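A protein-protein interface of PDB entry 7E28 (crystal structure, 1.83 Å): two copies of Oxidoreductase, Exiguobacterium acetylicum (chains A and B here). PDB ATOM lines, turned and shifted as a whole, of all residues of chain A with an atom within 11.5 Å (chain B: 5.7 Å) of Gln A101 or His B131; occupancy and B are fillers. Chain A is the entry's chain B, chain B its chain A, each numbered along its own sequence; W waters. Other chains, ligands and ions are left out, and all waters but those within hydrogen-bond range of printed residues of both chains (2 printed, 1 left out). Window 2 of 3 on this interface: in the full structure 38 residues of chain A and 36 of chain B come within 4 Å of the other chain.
No position is printed for both chains.
No residue of chain A comes within 4 Å of Ser B124.
Of chain A, only Val A100 (3.8 Å) and Gln A101 (3.8 Å) come within 4 Å of Val B127.
No residue of chain A comes within 4 Å of His B130.
No residue of chain A comes within 4 Å of Asp B132.
No residue of chain A comes within 4 Å of Leu B181.
Printed residues of chain A within 4 Å of Glu B173: Leu A99 (3.5 Å), Val A100 (2.8 Å) and Val A154 (3.3 Å).
Of the printed residues of chain A, Arg B128 touches Gln A101.
The nearest residue of chain B that does not touch Gln A101 is Glu B173 (4.5 Å).
The nearest residue of chain A that does not touch His B131 is Asp A102 (6.4 Å).
The nearest printed residue of chain B that does not touch Leu A99 is Val B127 (6.6 Å).
O of Val B127 lies within hydrogen-bond range of ND1 of His B131, 3.3 Å away.
The side-chain carboxylate (OD1) of Asp B129 is in salt-bridge range of the guanidinium group (NE) of Arg B128, 2.9 Å away.
The backbone carbonyl oxygen of Arg B128 lies within hydrogen-bond range of a ring nitrogen (ND1) of His B131, 3.2 Å away.
The backbone carbonyl oxygen (O) of His B131 is in hydrogen-bond range of the backbone NH (N) of Lys B180 (3.0 Å).
The backbone NH (N) of Leu B181 lies within hydrogen-bond range of the backbone carbonyl oxygen (O) of His B131, at 3.1 Å.
Of the 17 printed residues of chain A, 4 touch a printed residue of chain B.
Of the 15 printed residues of chain B, 4 touch a printed residue of chain A.
Among the printed residues, 7 pairs touch across the chains.
Among the printed residues, no Asp or Glu carboxylate lies within 4 Å of a Lys or Arg side-chain nitrogen of the other chain.
Among the printed residues, pairs that only touch across the chains: Leu A99 with Glu B173 (3.5 Å), Val A100 with Val B127 (3.8 Å), Gln A101 with Val B127 (3.8 Å), Gln A101 with Arg B128 (3.9 Å), Gln A101 with His B131 (3.8 Å) and Val A154 with Glu B173 (3.3 Å).
Water W1 lies within hydrogen-bond range of OE2 of Glu B173 (2.7 Å), OE1 of Gln A101 (2.8 Å) and N of Val A100 (3.3 Å).
Water W2 lies within hydrogen-bond range of O of Asp A98 (2.8 Å), OE1 of Glu B173 (2.9 Å) and N of Val A154 (2.9 Å).
OE2 of Glu B173 is in hydrogen-bond range of N of Val A100 (2.8 Å).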
ATOM      1  N   ASP A  96     -37.810  13.530  19.352  1.00  0.00           N
ATOM      2  CA  ASP A  96     -37.893  14.977  19.501  1.00  0.00           C
ATOM      3  C   ASP A  96     -37.741  15.623  18.139  1.00  0.00           C
ATOM      4  O   ASP A  96     -36.954  15.145  17.316  1.00  0.00           O
ATOM      5  CB  ASP A  96     -36.792  15.523  20.413  1.00  0.00           C
ATOM      6  CG  ASP A  96     -36.989  16.988  20.729  1.00  0.00           C
ATOM      7  OD1 ASP A  96     -38.117  17.333  21.135  1.00  0.00           O
ATOM      8  OD2 ASP A  96     -36.037  17.783  20.558  1.00  0.00           O
ATOM      9  N   PHE A  97     -38.476  16.717  17.925  1.00  0.00           N
ATOM     10  CA  PHE A  97     -38.295  17.604  16.781  1.00  0.00           C
ATOM     11  C   PHE A  97     -37.924  18.990  17.297  1.00  0.00           C
ATOM     12  O   PHE A  97     -38.696  19.606  18.045  1.00  0.00           O
ATOM     13  CB  PHE A  97     -39.550  17.669  15.905  1.00  0.00           C
ATOM     14  CG  PHE A  97     -39.813  16.402  15.137  1.00  0.00           C
ATOM     15  CD1 PHE A  97     -39.110  16.112  13.974  1.00  0.00           C
ATOM     16  CD2 PHE A  97     -40.760  15.493  15.585  1.00  0.00           C
ATOM     17  CE1 PHE A  97     -39.352  14.933  13.271  1.00  0.00           C
ATOM     18  CE2 PHE A  97     -41.002  14.320  14.889  1.00  0.00           C
ATOM     19  CZ  PHE A  97     -40.298  14.042  13.733  1.00  0.00           C
ATOM     20  N   ASP A  98     -36.746  19.471  16.891  1.00  0.00           N
ATOM     21  CA  ASP A  98     -36.213  20.764  17.310  1.00  0.00           C
ATOM     22  C   ASP A  98     -34.794  20.948  16.794  1.00  0.00           C
ATOM     23  O   ASP A  98     -33.994  20.000  16.811  1.00  0.00           O
ATOM     24  CB  ASP A  98     -36.207  20.907  18.825  1.00  0.00           C
ATOM     25  CG  ASP A  98     -37.330  21.787  19.338  1.00  0.00           C
ATOM     26  OD1 ASP A  98     -37.777  22.725  18.628  1.00  0.00           O
ATOM     27  OD2 ASP A  98     -37.744  21.557  20.485  1.00  0.00           O
ATOM     28  N   LEU A  99     -34.469  22.158  16.341  1.00  0.00           N
ATOM     29  CA  LEU A  99     -33.074  22.490  16.067  1.00  0.00           C
ATOM     30  C   LEU A  99     -32.237  22.296  17.331  1.00  0.00           C
ATOM     31  O   LEU A  99     -32.744  22.399  18.462  1.00  0.00           O
ATOM     32  CB  LEU A  99     -32.957  23.941  15.573  1.00  0.00           C
ATOM     33  CG  LEU A  99     -33.714  24.266  14.285  1.00  0.00           C
ATOM     34  CD1 LEU A  99     -33.668  25.807  14.013  1.00  0.00           C
ATOM     35  CD2 LEU A  99     -33.142  23.481  13.097  1.00  0.00           C
ATOM     36  N   VAL A 100     -30.946  21.978  17.143  1.00  0.00           N
ATOM     37  CA  VAL A 100     -30.091  21.770  18.314  1.00  0.00           C
ATOM     38  C   VAL A 100     -30.067  23.021  19.183  1.00  0.00           C
ATOM     39  O   VAL A 100     -30.160  22.937  20.420  1.00  0.00           O
ATOM     40  CB  VAL A 100     -28.673  21.335  17.906  1.00  0.00           C
ATOM     41  CG1 VAL A 100     -27.665  21.582  19.058  1.00  0.00           C
ATOM     42  CG2 VAL A 100     -28.673  19.858  17.518  1.00  0.00           C
ATOM     43  N   GLN A 101     -29.996  24.206  18.552  1.00  0.00           N
ATOM     44  CA  GLN A 101     -30.039  25.459  19.299  1.00  0.00           C
ATOM     45  C   GLN A 101     -31.306  25.617  20.129  1.00  0.00           C
ATOM     46  O   GLN A 101     -31.314  26.436  21.056  1.00  0.00           O
ATOM     47  CB  GLN A 101     -29.930  26.655  18.346  1.00  0.00           C
ATOM     48  CG  GLN A 101     -31.114  26.785  17.382  1.00  0.00           C
ATOM     49  CD  GLN A 101     -30.757  27.552  16.120  1.00  0.00           C
ATOM     50  OE1 GLN A 101     -29.857  27.151  15.371  1.00  0.00           O
ATOM     51  NE2 GLN A 101     -31.472  28.662  15.870  1.00  0.00           N
ATOM     52  N   ASP A 102     -32.379  24.886  19.815  1.00  0.00           N
ATOM     53  CA  ASP A 102     -33.690  25.088  20.439  1.00  0.00           C
ATOM     54  C   ASP A 102     -34.049  24.023  21.465  1.00  0.00           C
ATOM     55  O   ASP A 102     -35.131  24.107  22.067  1.00  0.00           O
ATOM     56  CB  ASP A 102     -34.777  25.120  19.363  1.00  0.00           C
ATOM     57  CG  ASP A 102     -34.756  26.413  18.569  1.00  0.00           C
ATOM     58  OD1 ASP A 102     -34.184  27.383  19.090  1.00  0.00           O
ATOM     59  OD2 ASP A 102     -35.277  26.443  17.433  1.00  0.00           O
ATOM     60  N   ILE A 103     -33.153  23.052  21.679  1.00  0.00           N
ATOM     61  CA  ILE A 103     -33.428  21.846  22.450  1.00  0.00           C
ATOM     62  C   ILE A 103     -33.770  22.157  23.905  1.00  0.00           C
ATOM     63  O   ILE A 103     -33.174  23.037  24.528  1.00  0.00           O
ATOM     64  CB  ILE A 103     -32.179  20.946  22.347  1.00  0.00           C
ATOM     65  CG1 ILE A 103     -32.178  20.143  21.047  1.00  0.00           C
ATOM     66  CG2 ILE A 103     -31.971  20.094  23.585  1.00  0.00           C
ATOM     67  CD1 ILE A 103     -33.389  19.325  20.850  1.00  0.00           C
ATOM     68  N   GLU A 104     -34.708  21.406  24.473  1.00  0.00           N
ATOM     69  CA  GLU A 104     -34.835  21.371  25.928  1.00  0.00           C
ATOM     70  C   GLU A 104     -33.863  20.320  26.457  1.00  0.00           C
ATOM     71  O   GLU A 104     -33.983  19.141  26.112  1.00  0.00           O
ATOM     72  CB  GLU A 104     -36.271  21.061  26.355  1.00  0.00           C
ATOM     73  CG  GLU A 104     -36.686  21.717  27.697  1.00  0.00           C
ATOM     74  CD  GLU A 104     -36.302  20.913  28.941  1.00  0.00           C
ATOM     75  OE1 GLU A 104     -35.288  21.248  29.599  1.00  0.00           O
ATOM     76  OE2 GLU A 104     -37.042  19.958  29.279  1.00  0.00           O
ATOM     77  N   LEU A 105     -32.892  20.733  27.280  1.00  0.00           N
ATOM     78  CA  LEU A 105     -31.827  19.809  27.662  1.00  0.00           C
ATOM     79  C   LEU A 105     -32.346  18.653  28.522  1.00  0.00           C
ATOM     80  O   LEU A 105     -31.985  17.498  28.289  1.00  0.00           O
ATOM     81  CB  LEU A 105     -30.697  20.547  28.369  1.00  0.00           C
ATOM     82  CG  LEU A 105     -29.531  20.763  27.401  1.00  0.00           C
ATOM     83  CD1 LEU A 105     -28.408  21.464  28.115  1.00  0.00           C
ATOM     84  CD2 LEU A 105     -29.057  19.459  26.754  1.00  0.00           C
ATOM     85  N   GLY A 106     -33.207  18.940  29.507  1.00  0.00           N
ATOM     86  CA  GLY A 106     -33.733  17.876  30.350  1.00  0.00           C
ATOM     87  C   GLY A 106     -34.368  16.760  29.541  1.00  0.00           C
ATOM     88  O   GLY A 106     -34.152  15.572  29.809  1.00  0.00           O
ATOM     89  N   ILE A 108     -33.695  16.044  26.319  1.00  0.00           N
ATOM     90  CA  ILE A 108     -32.623  15.382  25.581  1.00  0.00           C
ATOM     91  C   ILE A 108     -31.825  14.456  26.492  1.00  0.00           C
ATOM     92  O   ILE A 108     -31.451  13.348  26.093  1.00  0.00           O
ATOM     93  CB  ILE A 108     -31.708  16.424  24.907  1.00  0.00           C
ATOM     94  CG1 ILE A 108     -32.417  17.110  23.723  1.00  0.00           C
ATOM     95  CG2 ILE A 108     -30.377  15.801  24.494  1.00  0.00           C
ATOM     96  CD1 ILE A 108     -33.414  16.268  22.976  1.00  0.00           C
ATOM     97  N   PRO A 151     -33.631  15.865   9.094  1.00  0.00           N
ATOM     98  CA  PRO A 151     -33.491  17.252   9.560  1.00  0.00           C
ATOM     99  C   PRO A 151     -34.484  17.558  10.666  1.00  0.00           C
ATOM    100  O   PRO A 151     -35.627  17.095  10.652  1.00  0.00           O
ATOM    101  CB  PRO A 151     -33.765  18.079   8.297  1.00  0.00           C
ATOM    102  CG  PRO A 151     -33.386  17.164   7.160  1.00  0.00           C
ATOM    103  CD  PRO A 151     -33.774  15.780   7.627  1.00  0.00           C
ATOM    104  N   ASN A 152     -34.029  18.330  11.644  1.00  0.00           N
ATOM    105  CA  ASN A 152     -34.791  18.751  12.815  1.00  0.00           C
ATOM    106  C   ASN A 152     -34.905  17.661  13.864  1.00  0.00           C
ATOM    107  O   ASN A 152     -35.598  17.871  14.865  1.00  0.00           O
ATOM    108  CB  ASN A 152     -36.207  19.221  12.471  1.00  0.00           C
ATOM    109  CG  ASN A 152     -36.263  20.677  12.258  1.00  0.00           C
ATOM    110  OD1 ASN A 152     -35.878  21.182  11.195  1.00  0.00           O
ATOM    111  ND2 ASN A 152     -36.721  21.392  13.276  1.00  0.00           N
ATOM    112  N   ALA A 153     -34.274  16.507  13.673  1.00  0.00           N
ATOM    113  CA  ALA A 153     -34.273  15.459  14.695  1.00  0.00           C
ATOM    114  C   ALA A 153     -32.868  14.890  14.801  1.00  0.00           C
ATOM    115  O   ALA A 153     -32.660  13.676  14.825  1.00  0.00           O
ATOM    116  CB  ALA A 153     -35.306  14.377  14.394  1.00  0.00           C
ATOM    117  N   VAL A 154     -31.886  15.795  14.867  1.00  0.00           N
ATOM    118  CA  VAL A 154     -30.478  15.411  14.835  1.00  0.00           C
ATOM    119  C   VAL A 154     -30.147  14.519  16.031  1.00  0.00           C
ATOM    120  O   VAL A 154     -29.535  13.454  15.886  1.00  0.00           O
ATOM    121  CB  VAL A 154     -29.578  16.664  14.803  1.00  0.00           C
ATOM    122  CG1 VAL A 154     -28.128  16.281  15.098  1.00  0.00           C
ATOM    123  CG2 VAL A 154     -29.675  17.385  13.441  1.00  0.00           C
ATOM    124  N   THR A 155     -30.563  14.940  17.228  1.00  0.00           N
ATOM    125  CA  THR A 155     -30.188  14.235  18.448  1.00  0.00           C
ATOM    126  C   THR A 155     -30.884  12.877  18.530  1.00  0.00           C
ATOM    127  O   THR A 155     -30.256  11.864  18.857  1.00  0.00           O
ATOM    128  CB  THR A 155     -30.513  15.103  19.669  1.00  0.00           C
ATOM    129  OG1 THR A 155     -29.938  16.421  19.512  1.00  0.00           O
ATOM    130  CG2 THR A 155     -29.981  14.454  20.939  1.00  0.00           C
ATOM    131  N   SER B 124     -24.748  21.150  22.803  1.00  0.00           N
ATOM    132  CA  SER B 124     -26.059  21.800  22.758  1.00  0.00           C
ATOM    133  C   SER B 124     -26.015  23.183  23.404  1.00  0.00           C
ATOM    134  O   SER B 124     -26.648  24.130  22.917  1.00  0.00           O
ATOM    135  CB  SER B 124     -27.099  20.913  23.448  1.00  0.00           C
ATOM    136  OG  SER B 124     -27.241  19.661  22.782  1.00  0.00           O
ATOM    137  N   PHE B 126     -23.231  25.146  23.765  1.00  0.00           N
ATOM    138  CA  PHE B 126     -22.415  26.014  22.914  1.00  0.00           C
ATOM    139  C   PHE B 126     -23.205  26.503  21.697  1.00  0.00           C
ATOM    140  O   PHE B 126     -23.243  27.708  21.399  1.00  0.00           O
ATOM    141  CB  PHE B 126     -21.154  25.256  22.487  1.00  0.00           C
ATOM    142  CG  PHE B 126     -20.101  26.131  21.889  1.00  0.00           C
ATOM    143  CD1 PHE B 126     -19.426  27.056  22.669  1.00  0.00           C
ATOM    144  CD2 PHE B 126     -19.765  26.009  20.542  1.00  0.00           C
ATOM    145  CE1 PHE B 126     -18.441  27.884  22.105  1.00  0.00           C
ATOM    146  CE2 PHE B 126     -18.785  26.822  19.979  1.00  0.00           C
ATOM    147  CZ  PHE B 126     -18.122  27.755  20.765  1.00  0.00           C
ATOM    148  N   VAL B 127     -23.867  25.575  20.999  1.00  0.00           N
ATOM    149  CA  VAL B 127     -24.665  25.928  19.826  1.00  0.00           C
ATOM    150  C   VAL B 127     -25.753  26.927  20.204  1.00  0.00           C
ATOM    151  O   VAL B 127     -25.995  27.904  19.478  1.00  0.00           O
ATOM    152  CB  VAL B 127     -25.262  24.663  19.181  1.00  0.00           C
ATOM    153  CG1 VAL B 127     -26.340  25.045  18.154  1.00  0.00           C
ATOM    154  CG2 VAL B 127     -24.171  23.840  18.524  1.00  0.00           C
ATOM    155  N   ARG B 128     -26.426  26.692  21.338  1.00  0.00           N
ATOM    156  CA  ARG B 128     -27.463  27.613  21.802  1.00  0.00           C
ATOM    157  C   ARG B 128     -26.946  29.048  21.806  1.00  0.00           C
ATOM    158  O   ARG B 128     -27.572  29.956  21.243  1.00  0.00           O
ATOM    159  CB  ARG B 128     -27.947  27.205  23.203  1.00  0.00           C
ATOM    160  CG  ARG B 128     -29.102  28.080  23.757  1.00  0.00           C
ATOM    161  CD  ARG B 128     -29.410  27.798  25.246  1.00  0.00           C
ATOM    162  NE  ARG B 128     -28.282  28.145  26.108  1.00  0.00           N
ATOM    163  CZ  ARG B 128     -28.217  27.902  27.413  1.00  0.00           C
ATOM    164  NH1 ARG B 128     -29.220  27.303  28.050  1.00  0.00           N
ATOM    165  NH2 ARG B 128     -27.140  28.275  28.079  1.00  0.00           N
ATOM    166  N   ASP B 129     -25.767  29.253  22.383  1.00  0.00           N
ATOM    167  CA  ASP B 129     -25.249  30.590  22.637  1.00  0.00           C
ATOM    168  C   ASP B 129     -24.400  31.156  21.499  1.00  0.00           C
ATOM    169  O   ASP B 129     -24.110  32.353  21.520  1.00  0.00           O
ATOM    170  CB  ASP B 129     -24.427  30.571  23.940  1.00  0.00           C
ATOM    171  CG  ASP B 129     -25.258  30.145  25.140  1.00  0.00           C
ATOM    172  OD1 ASP B 129     -26.504  30.128  25.003  1.00  0.00           O
ATOM    173  OD2 ASP B 129     -24.682  29.814  26.213  1.00  0.00           O
ATOM    174  N   HIS B 130     -24.004  30.348  20.505  1.00  0.00           N
ATOM    175  CA  HIS B 130     -22.994  30.755  19.541  1.00  0.00           C
ATOM    176  C   HIS B 130     -23.380  30.506  18.087  1.00  0.00           C
ATOM    177  O   HIS B 130     -22.557  30.767  17.196  1.00  0.00           O
ATOM    178  CB  HIS B 130     -21.658  30.039  19.820  1.00  0.00           C
ATOM    179  CG  HIS B 130     -21.074  30.345  21.161  1.00  0.00           C
ATOM    180  ND1 HIS B 130     -21.494  29.722  22.314  1.00  0.00           N
ATOM    181  CD2 HIS B 130     -20.099  31.209  21.533  1.00  0.00           C
ATOM    182  CE1 HIS B 130     -20.812  30.195  23.342  1.00  0.00           C
ATOM    183  NE2 HIS B 130     -19.952  31.092  22.894  1.00  0.00           N
ATOM    184  N   HIS B 131     -24.595  30.020  17.813  1.00  0.00           N
ATOM    185  CA  HIS B 131     -24.929  29.651  16.441  1.00  0.00           C
ATOM    186  C   HIS B 131     -24.831  30.845  15.489  1.00  0.00           C
ATOM    187  O   HIS B 131     -24.527  30.671  14.301  1.00  0.00           O
ATOM    188  CB  HIS B 131     -26.326  29.027  16.393  1.00  0.00           C
ATOM    189  CG  HIS B 131     -27.438  29.976  16.749  1.00  0.00           C
ATOM    190  ND1 HIS B 131     -27.962  30.068  18.027  1.00  0.00           N
ATOM    191  CD2 HIS B 131     -28.146  30.847  15.985  1.00  0.00           C
ATOM    192  CE1 HIS B 131     -28.928  30.970  18.039  1.00  0.00           C
ATOM    193  NE2 HIS B 131     -29.063  31.454  16.814  1.00  0.00           N
ATOM    194  N   ASP B 132     -25.060  32.058  15.993  1.00  0.00           N
ATOM    195  CA  ASP B 132     -25.098  33.264  15.172  1.00  0.00           C
ATOM    196  C   ASP B 132     -23.868  34.149  15.384  1.00  0.00           C
ATOM    197  O   ASP B 132     -23.913  35.355  15.113  1.00  0.00           O
ATOM    198  CB  ASP B 132     -26.383  34.052  15.465  1.00  0.00           C
ATOM    199  CG  ASP B 132     -26.691  35.107  14.407  1.00  0.00           C
ATOM    200  OD1 ASP B 132     -27.353  36.115  14.744  1.00  0.00           O
ATOM    201  OD2 ASP B 132     -26.254  34.935  13.243  1.00  0.00           O
ATOM    202  N   ILE B 133     -22.765  33.584  15.862  1.00  0.00           N
ATOM    203  CA  ILE B 133     -21.576  34.357  16.191  1.00  0.00           C
ATOM    204  C   ILE B 133     -20.467  33.993  15.214  1.00  0.00           C
ATOM    205  O   ILE B 133     -20.064  32.827  15.107  1.00  0.00           O
ATOM    206  CB  ILE B 133     -21.147  34.137  17.643  1.00  0.00           C
ATOM    207  CG1 ILE B 133     -22.262  34.585  18.588  1.00  0.00           C
ATOM    208  CG2 ILE B 133     -19.851  34.869  17.922  1.00  0.00           C
ATOM    209  CD1 ILE B 133     -21.803  34.734  20.004  1.00  0.00           C
ATOM    210  N   THR B 136     -16.930  31.236  15.065  1.00  0.00           N
ATOM    211  CA  THR B 136     -16.989  30.212  16.099  1.00  0.00           C
ATOM    212  C   THR B 136     -16.993  28.825  15.455  1.00  0.00           C
ATOM    213  O   THR B 136     -17.534  28.635  14.357  1.00  0.00           O
ATOM    214  CB  THR B 136     -18.215  30.406  17.006  1.00  0.00           C
ATOM    215  OG1 THR B 136     -19.441  30.314  16.256  1.00  0.00           O
ATOM    216  CG2 THR B 136     -18.156  31.766  17.690  1.00  0.00           C
ATOM    217  N   GLU B 173     -27.246  20.965   9.598  1.00  0.00           N
ATOM    218  CA  GLU B 173     -28.314  21.836  10.073  1.00  0.00           C
ATOM    219  C   GLU B 173     -27.851  23.294  10.145  1.00  0.00           C
ATOM    220  O   GLU B 173     -28.604  24.218   9.798  1.00  0.00           O
ATOM    221  CB  GLU B 173     -28.789  21.339  11.436  1.00  0.00           C
ATOM    222  CG  GLU B 173     -29.716  22.251  12.205  1.00  0.00           C
ATOM    223  CD  GLU B 173     -30.184  21.596  13.481  1.00  0.00           C
ATOM    224  OE1 GLU B 173     -30.824  20.511  13.399  1.00  0.00           O
ATOM    225  OE2 GLU B 173     -29.889  22.132  14.570  1.00  0.00           O
ATOM    226  N   LEU B 174     -26.622  23.519  10.607  1.00  0.00           N
ATOM    227  CA  LEU B 174     -26.079  24.872  10.650  1.00  0.00           C
ATOM    228  C   LEU B 174     -25.821  25.413   9.245  1.00  0.00           C
ATOM    229  O   LEU B 174     -26.309  26.490   8.882  1.00  0.00           O
ATOM    230  CB  LEU B 174     -24.796  24.879  11.480  1.00  0.00           C
ATOM    231  CG  LEU B 174     -24.988  24.557  12.964  1.00  0.00           C
ATOM    232  CD1 LEU B 174     -23.643  24.355  13.610  1.00  0.00           C
ATOM    233  CD2 LEU B 174     -25.788  25.658  13.675  1.00  0.00           C
ATOM    234  N   ALA B 179     -26.271  29.377   9.384  1.00  0.00           N
ATOM    235  CA  ALA B 179     -25.691  29.776  10.658  1.00  0.00           C
ATOM    236  C   ALA B 179     -24.246  30.240  10.477  1.00  0.00           C
ATOM    237  O   ALA B 179     -23.571  29.898   9.503  1.00  0.00           O
ATOM    238  CB  ALA B 179     -25.721  28.609  11.655  1.00  0.00           C
ATOM    239  N   LYS B 180     -23.750  30.988  11.463  1.00  0.00           N
ATOM    240  CA  LYS B 180     -22.360  31.418  11.379  1.00  0.00           C
ATOM    241  C   LYS B 180     -21.415  30.397  12.014  1.00  0.00           C
ATOM    242  O   LYS B 180     -20.313  30.168  11.502  1.00  0.00           O
ATOM    243  CB  LYS B 180     -22.216  32.803  12.008  1.00  0.00           C
ATOM    244  CG  LYS B 180     -23.199  33.822  11.422  1.00  0.00           C
ATOM    245  CD  LYS B 180     -22.504  35.080  10.941  1.00  0.00           C
ATOM    246  CE  LYS B 180     -23.504  36.214  10.617  1.00  0.00           C
ATOM    247  NZ  LYS B 180     -24.088  36.845  11.845  1.00  0.00           N
ATOM    248  N   LEU B 181     -21.834  29.775  13.118  1.00  0.00           N
ATOM    249  CA  LEU B 181     -21.060  28.711  13.755  1.00  0.00           C
ATOM    250  C   LEU B 181     -20.849  27.536  12.798  1.00  0.00           C
ATOM    251  O   LEU B 181     -21.761  27.157  12.055  1.00  0.00           O
ATOM    252  CB  LEU B 181     -21.778  28.257  15.027  1.00  0.00           C
ATOM    253  CG  LEU B 181     -21.347  26.944  15.692  1.00  0.00           C
ATOM    254  CD1 LEU B 181     -19.993  27.072  16.384  1.00  0.00           C
ATOM    255  CD2 LEU B 181     -22.431  26.553  16.672  1.00  0.00           C
HETATM  256  O   HOH W   1     -29.140  24.455  15.796  1.00  0.00           O
HETATM  257  O   HOH W   2     -32.061  18.683  15.311  1.00  0.00           O
